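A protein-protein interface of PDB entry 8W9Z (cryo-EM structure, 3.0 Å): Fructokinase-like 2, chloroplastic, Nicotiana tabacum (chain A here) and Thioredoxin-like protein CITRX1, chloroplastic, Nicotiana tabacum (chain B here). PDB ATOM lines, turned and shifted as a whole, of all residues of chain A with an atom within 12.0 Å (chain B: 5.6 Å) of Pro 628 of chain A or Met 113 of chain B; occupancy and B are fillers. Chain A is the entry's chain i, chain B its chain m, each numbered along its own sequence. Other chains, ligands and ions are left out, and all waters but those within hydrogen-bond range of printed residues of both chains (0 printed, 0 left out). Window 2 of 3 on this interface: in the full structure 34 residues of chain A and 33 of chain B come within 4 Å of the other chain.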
ATOM      1  N   TYR A 560      37.753  -5.567  22.761  1.00  0.00           N
ATOM      2  CA  TYR A 560      36.661  -6.539  22.790  1.00  0.00           C
ATOM      3  C   TYR A 560      37.116  -7.890  23.326  1.00  0.00           C
ATOM      4  O   TYR A 560      36.280  -8.787  23.495  1.00  0.00           O
ATOM      5  CB  TYR A 560      35.999  -6.764  21.421  1.00  0.00           C
ATOM      6  CG  TYR A 560      35.658  -5.510  20.652  1.00  0.00           C
ATOM      7  CD1 TYR A 560      35.271  -4.348  21.303  1.00  0.00           C
ATOM      8  CD2 TYR A 560      35.720  -5.492  19.265  1.00  0.00           C
ATOM      9  CE1 TYR A 560      34.956  -3.205  20.595  1.00  0.00           C
ATOM     10  CE2 TYR A 560      35.407  -4.355  18.550  1.00  0.00           C
ATOM     11  CZ  TYR A 560      35.028  -3.215  19.218  1.00  0.00           C
ATOM     12  OH  TYR A 560      34.715  -2.078  18.510  1.00  0.00           O
ATOM     13  N   PRO A 618      37.514   0.158  14.828  1.00  0.00           N
ATOM     14  CA  PRO A 618      38.053   1.068  13.812  1.00  0.00           C
ATOM     15  C   PRO A 618      38.928   2.139  14.442  1.00  0.00           C
ATOM     16  O   PRO A 618      38.652   2.630  15.539  1.00  0.00           O
ATOM     17  CB  PRO A 618      36.798   1.669  13.172  1.00  0.00           C
ATOM     18  CG  PRO A 618      35.750   1.549  14.223  1.00  0.00           C
ATOM     19  CD  PRO A 618      36.051   0.272  14.951  1.00  0.00           C
ATOM     20  N   MET A 622      37.999   6.065  10.104  1.00  0.00           N
ATOM     21  CA  MET A 622      37.042   4.975   9.959  1.00  0.00           C
ATOM     22  C   MET A 622      36.155   5.228   8.747  1.00  0.00           C
ATOM     23  O   MET A 622      35.425   6.225   8.700  1.00  0.00           O
ATOM     24  CB  MET A 622      36.199   4.819  11.226  1.00  0.00           C
ATOM     25  CG  MET A 622      35.701   6.129  11.815  1.00  0.00           C
ATOM     26  SD  MET A 622      34.725   5.892  13.314  1.00  0.00           S
ATOM     27  CE  MET A 622      33.390   4.874  12.692  1.00  0.00           C
ATOM     28  N   ASP A 624      34.865   2.064   7.186  1.00  0.00           N
ATOM     29  CA  ASP A 624      34.381   0.715   6.944  1.00  0.00           C
ATOM     30  C   ASP A 624      32.855   0.680   6.957  1.00  0.00           C
ATOM     31  O   ASP A 624      32.189   1.577   7.483  1.00  0.00           O
ATOM     32  CB  ASP A 624      34.944  -0.247   7.992  1.00  0.00           C
ATOM     33  CG  ASP A 624      34.752  -1.704   7.617  1.00  0.00           C
ATOM     34  OD1 ASP A 624      34.289  -1.975   6.488  1.00  0.00           O
ATOM     35  OD2 ASP A 624      35.065  -2.580   8.450  1.00  0.00           O
ATOM     36  N   ASP A 625      32.304  -0.374   6.358  1.00  0.00           N
ATOM     37  CA  ASP A 625      30.859  -0.557   6.339  1.00  0.00           C
ATOM     38  C   ASP A 625      30.332  -0.728   7.758  1.00  0.00           C
ATOM     39  O   ASP A 625      30.884  -1.497   8.551  1.00  0.00           O
ATOM     40  CB  ASP A 625      30.492  -1.770   5.483  1.00  0.00           C
ATOM     41  CG  ASP A 625      29.001  -1.872   5.223  1.00  0.00           C
ATOM     42  OD1 ASP A 625      28.266  -0.923   5.566  1.00  0.00           O
ATOM     43  OD2 ASP A 625      28.565  -2.905   4.673  1.00  0.00           O
ATOM     44  N   VAL A 626      29.260  -0.009   8.074  1.00  0.00           N
ATOM     45  CA  VAL A 626      28.724   0.027   9.431  1.00  0.00           C
ATOM     46  C   VAL A 626      27.832  -1.193   9.637  1.00  0.00           C
ATOM     47  O   VAL A 626      26.778  -1.318   9.010  1.00  0.00           O
ATOM     48  CB  VAL A 626      27.957   1.326   9.697  1.00  0.00           C
ATOM     49  CG1 VAL A 626      27.420   1.341  11.121  1.00  0.00           C
ATOM     50  CG2 VAL A 626      28.850   2.530   9.444  1.00  0.00           C
ATOM     51  N   VAL A 627      28.257  -2.095  10.513  1.00  0.00           N
ATOM     52  CA  VAL A 627      27.399  -3.215  10.919  1.00  0.00           C
ATOM     53  C   VAL A 627      26.239  -2.672  11.744  1.00  0.00           C
ATOM     54  O   VAL A 627      26.449  -1.768  12.574  1.00  0.00           O
ATOM     55  CB  VAL A 627      28.215  -4.243  11.710  1.00  0.00           C
ATOM     56  CG1 VAL A 627      27.361  -5.438  12.105  1.00  0.00           C
ATOM     57  CG2 VAL A 627      29.427  -4.689  10.905  1.00  0.00           C
ATOM     58  N   PRO A 628      25.009  -3.161  11.550  1.00  0.00           N
ATOM     59  CA  PRO A 628      23.862  -2.591  12.279  1.00  0.00           C
ATOM     60  C   PRO A 628      23.991  -2.619  13.797  1.00  0.00           C
ATOM     61  O   PRO A 628      23.215  -1.929  14.470  1.00  0.00           O
ATOM     62  CB  PRO A 628      22.688  -3.461  11.813  1.00  0.00           C
ATOM     63  CG  PRO A 628      23.089  -3.919  10.456  1.00  0.00           C
ATOM     64  CD  PRO A 628      24.581  -4.110  10.507  1.00  0.00           C
ATOM     65  N   ASP A 629      24.932  -3.379  14.359  1.00  0.00           N
ATOM     66  CA  ASP A 629      25.063  -3.487  15.804  1.00  0.00           C
ATOM     67  C   ASP A 629      26.418  -3.059  16.352  1.00  0.00           C
ATOM     68  O   ASP A 629      26.508  -2.774  17.551  1.00  0.00           O
ATOM     69  CB  ASP A 629      24.781  -4.927  16.261  1.00  0.00           C
ATOM     70  CG  ASP A 629      23.335  -5.332  16.051  1.00  0.00           C
ATOM     71  OD1 ASP A 629      22.520  -4.464  15.677  1.00  0.00           O
ATOM     72  OD2 ASP A 629      23.010  -6.518  16.260  1.00  0.00           O
ATOM     73  N   ASP A 630      27.459  -2.999  15.529  1.00  0.00           N
ATOM     74  CA  ASP A 630      28.790  -2.620  15.994  1.00  0.00           C
ATOM     75  C   ASP A 630      29.614  -2.182  14.788  1.00  0.00           C
ATOM     76  O   ASP A 630      29.078  -1.940  13.702  1.00  0.00           O
ATOM     77  CB  ASP A 630      29.455  -3.771  16.754  1.00  0.00           C
ATOM     78  CG  ASP A 630      29.746  -4.964  15.867  1.00  0.00           C
ATOM     79  OD1 ASP A 630      28.907  -5.279  14.998  1.00  0.00           O
ATOM     80  OD2 ASP A 630      30.817  -5.583  16.035  1.00  0.00           O
ATOM     81  N   HIS A 631      30.924  -2.060  14.987  1.00  0.00           N
ATOM     82  CA  HIS A 631      31.840  -1.690  13.913  1.00  0.00           C
ATOM     83  C   HIS A 631      33.202  -2.286  14.225  1.00  0.00           C
ATOM     84  O   HIS A 631      33.768  -2.011  15.287  1.00  0.00           O
ATOM     85  CB  HIS A 631      31.931  -0.169  13.769  1.00  0.00           C
ATOM     86  CG  HIS A 631      32.201   0.291  12.371  1.00  0.00           C
ATOM     87  ND1 HIS A 631      32.330   1.622  12.038  1.00  0.00           N
ATOM     88  CD2 HIS A 631      32.359  -0.402  11.218  1.00  0.00           C
ATOM     89  CE1 HIS A 631      32.560   1.729  10.741  1.00  0.00           C
ATOM     90  NE2 HIS A 631      32.581   0.515  10.220  1.00  0.00           N
ATOM     91  N   GLY A 632      33.724  -3.101  13.311  1.00  0.00           N
ATOM     92  CA  GLY A 632      34.986  -3.775  13.544  1.00  0.00           C
ATOM     93  C   GLY A 632      35.787  -4.051  12.289  1.00  0.00           C
ATOM     94  O   GLY A 632      35.221  -4.344  11.232  1.00  0.00           O
ATOM     95  N   ALA B 108      28.984   0.612  23.580  1.00  0.00           N
ATOM     96  CA  ALA B 108      29.036   2.060  23.414  1.00  0.00           C
ATOM     97  C   ALA B 108      28.770   2.464  21.970  1.00  0.00           C
ATOM     98  O   ALA B 108      28.123   3.487  21.713  1.00  0.00           O
ATOM     99  CB  ALA B 108      30.388   2.594  23.883  1.00  0.00           C
ATOM    100  N   GLN B 109      29.253   1.671  21.011  1.00  0.00           N
ATOM    101  CA  GLN B 109      29.040   1.996  19.604  1.00  0.00           C
ATOM    102  C   GLN B 109      27.559   1.945  19.246  1.00  0.00           C
ATOM    103  O   GLN B 109      27.030   2.858  18.600  1.00  0.00           O
ATOM    104  CB  GLN B 109      29.846   1.046  18.719  1.00  0.00           C
ATOM    105  CG  GLN B 109      31.345   1.112  18.950  1.00  0.00           C
ATOM    106  CD  GLN B 109      32.122   0.234  17.991  1.00  0.00           C
ATOM    107  OE1 GLN B 109      31.546  -0.400  17.107  1.00  0.00           O
ATOM    108  NE2 GLN B 109      33.437   0.192  18.160  1.00  0.00           N
ATOM    109  N   GLU B 110      26.867   0.885  19.668  1.00  0.00           N
ATOM    110  CA  GLU B 110      25.444   0.792  19.361  1.00  0.00           C
ATOM    111  C   GLU B 110      24.632   1.799  20.167  1.00  0.00           C
ATOM    112  O   GLU B 110      23.596   2.273  19.691  1.00  0.00           O
ATOM    113  CB  GLU B 110      24.937  -0.631  19.593  1.00  0.00           C
ATOM    114  CG  GLU B 110      24.884  -1.065  21.040  1.00  0.00           C
ATOM    115  CD  GLU B 110      24.305  -2.454  21.198  1.00  0.00           C
ATOM    116  OE1 GLU B 110      24.587  -3.318  20.342  1.00  0.00           O
ATOM    117  OE2 GLU B 110      23.557  -2.676  22.172  1.00  0.00           O
ATOM    118  N   LEU B 111      25.093   2.166  21.365  1.00  0.00           N
ATOM    119  CA  LEU B 111      24.422   3.233  22.102  1.00  0.00           C
ATOM    120  C   LEU B 111      24.550   4.565  21.375  1.00  0.00           C
ATOM    121  O   LEU B 111      23.591   5.342  21.318  1.00  0.00           O
ATOM    122  CB  LEU B 111      24.984   3.337  23.518  1.00  0.00           C
ATOM    123  CG  LEU B 111      24.478   2.289  24.510  1.00  0.00           C
ATOM    124  CD1 LEU B 111      25.036   2.551  25.897  1.00  0.00           C
ATOM    125  CD2 LEU B 111      22.959   2.272  24.536  1.00  0.00           C
ATOM    126  N   GLU B 112      25.724   4.844  20.805  1.00  0.00           N
ATOM    127  CA  GLU B 112      25.891   6.066  20.025  1.00  0.00           C
ATOM    128  C   GLU B 112      25.041   6.029  18.760  1.00  0.00           C
ATOM    129  O   GLU B 112      24.472   7.050  18.355  1.00  0.00           O
ATOM    130  CB  GLU B 112      27.367   6.274  19.686  1.00  0.00           C
ATOM    131  CG  GLU B 112      27.686   7.609  19.026  1.00  0.00           C
ATOM    132  CD  GLU B 112      27.570   7.563  17.514  1.00  0.00           C
ATOM    133  OE1 GLU B 112      27.505   6.448  16.955  1.00  0.00           O
ATOM    134  OE2 GLU B 112      27.545   8.642  16.886  1.00  0.00           O
ATOM    135  N   MET B 113      24.946   4.859  18.122  1.00  0.00           N
ATOM    136  CA  MET B 113      24.100   4.735  16.937  1.00  0.00           C
ATOM    137  C   MET B 113      22.630   4.944  17.285  1.00  0.00           C
ATOM    138  O   MET B 113      21.867   5.502  16.488  1.00  0.00           O
ATOM    139  CB  MET B 113      24.308   3.372  16.281  1.00  0.00           C
ATOM    140  CG  MET B 113      23.478   3.155  15.026  1.00  0.00           C
ATOM    141  SD  MET B 113      23.741   1.532  14.287  1.00  0.00           S
ATOM    142  CE  MET B 113      22.637   1.620  12.880  1.00  0.00           C
ATOM    143  N   LEU B 114      22.213   4.497  18.471  1.00  0.00           N
ATOM    144  CA  LEU B 114      20.840   4.722  18.905  1.00  0.00           C
ATOM    145  C   LEU B 114      20.607   6.186  19.258  1.00  0.00           C
ATOM    146  O   LEU B 114      19.528   6.731  18.997  1.00  0.00           O
ATOM    147  CB  LEU B 114      20.517   3.823  20.098  1.00  0.00           C
ATOM    148  CG  LEU B 114      19.098   3.907  20.660  1.00  0.00           C
ATOM    149  CD1 LEU B 114      18.094   3.406  19.638  1.00  0.00           C
ATOM    150  CD2 LEU B 114      18.989   3.124  21.959  1.00  0.00           C
ATOM    151  N   ALA B 115      21.608   6.839  19.853  1.00  0.00           N
ATOM    152  CA  ALA B 115      21.456   8.236  20.244  1.00  0.00           C
ATOM    153  C   ALA B 115      21.473   9.167  19.039  1.00  0.00           C
ATOM    154  O   ALA B 115      20.855  10.238  19.079  1.00  0.00           O
ATOM    155  CB  ALA B 115      22.556   8.628  21.230  1.00  0.00           C
ATOM    156  N   VAL B 116      22.172   8.789  17.964  1.00  0.00           N
ATOM    157  CA  VAL B 116      22.190   9.633  16.775  1.00  0.00           C
ATOM    158  C   VAL B 116      20.846   9.613  16.059  1.00  0.00           C
ATOM    159  O   VAL B 116      20.571  10.498  15.239  1.00  0.00           O
ATOM    160  CB  VAL B 116      23.325   9.211  15.822  1.00  0.00           C
ATOM    161  CG1 VAL B 116      22.881   8.071  14.919  1.00  0.00           C
ATOM    162  CG2 VAL B 116      23.801  10.401  15.000  1.00  0.00           C
ATOM    163  N   GLU B 117      19.995   8.627  16.349  1.00  0.00           N
ATOM    164  CA  GLU B 117      18.647   8.591  15.800  1.00  0.00           C
ATOM    165  C   GLU B 117      17.635   9.321  16.670  1.00  0.00           C
ATOM    166  O   GLU B 117      16.606   9.773  16.156  1.00  0.00           O
ATOM    167  CB  GLU B 117      18.193   7.140  15.603  1.00  0.00           C
ATOM    168  CG  GLU B 117      19.012   6.363  14.584  1.00  0.00           C
ATOM    169  CD  GLU B 117      18.789   6.841  13.162  1.00  0.00           C
ATOM    170  OE1 GLU B 117      17.748   7.482  12.901  1.00  0.00           O
ATOM    171  OE2 GLU B 117      19.654   6.575  12.302  1.00  0.00           O
ATOM    172  N   ILE B 167      20.136  -3.720  19.202  1.00  0.00           N
ATOM    173  CA  ILE B 167      19.556  -2.385  19.147  1.00  0.00           C
ATOM    174  C   ILE B 167      18.045  -2.441  18.958  1.00  0.00           C
ATOM    175  O   ILE B 167      17.339  -1.497  19.335  1.00  0.00           O
ATOM    176  CB  ILE B 167      20.231  -1.563  18.032  1.00  0.00           C
ATOM    177  CG1 ILE B 167      19.830  -0.089  18.120  1.00  0.00           C
ATOM    178  CG2 ILE B 167      19.896  -2.134  16.661  1.00  0.00           C
ATOM    179  CD1 ILE B 167      20.519   0.794  17.101  1.00  0.00           C
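Along chain B the printed residues that touch a printed residue of chain A span positions 109 to 167. Printed residues of chain A that touch a printed residue of chain B: Tyr 560, Pro 628, Asp 629, Asp 630 and His 631.
Of the printed residues of chain B, Tyr 560 of chain A touches Gln 109. Printed residues of chain B within 4 Å of Pro 628 of chain A: Met 113 (3.5 Å) and Ile 167 (3.98 Å). Printed residues of chain B within 4 Å of Asp 629 of chain A: Glu 110 and Ile 167. Of the printed residues of chain B, Asp 630 of chain A touches Gln 109 (3.5 Å). Printed residues of chain A within 4 Å of Glu 110 of chain B: Asp 629. No residue of chain A comes within 4 Å of Glu 112 of chain B. Met 113 of chain B touches just one residue of chain A: Pro 628. No residue of chain A comes within 4 Å of Leu 114 of chain B. Ala 115 of chain B touches none of the printed residues of chain A. No residue of chain A comes within 4 Å of Glu 117 of chain B. The nearest printed residue of chain B that does not touch His 631 of chain A is Glu 110 of chain B (6.9 Å).
The side-chain hydroxyl (OH) of Tyr 560 of chain A sits at hydrogen-bond distance from the backbone carbonyl oxygen (O) of His 631 of chain A (3.4 Å). NE2 of His 631 of chain A sits at hydrogen-bond distance from O of Asp 624 of chain A (3.0 Å). NE2 of His 631 of chain A lies within hydrogen-bond range of O of Asp 625 of chain A.
Among the printed residues, pairs that only touch across the chains: Pro 628 of chain A with Ile 167 of chain B (3.98 Å), Asp 629 of chain A with Ile 167 of chain B (3.6 Å) and Asp 630 of chain A with Gln 109 of chain B (3.5 Å).
NE2 of Gln 109 of chain B is in hydrogen-bond range of OH of Tyr 560 of chain A. N of His 631 of chain A is in hydrogen-bond range of OE1 of Gln 109 of chain B. O of Pro 628 of chain A lies close to SD of Met 113 of chain B, at 3.5 Å. The backbone carbonyl oxygen (O) of Asp 629 of chain A lies close to the side-chain carboxylate (OE1) of Glu 110 of chain B (3.4 Å).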
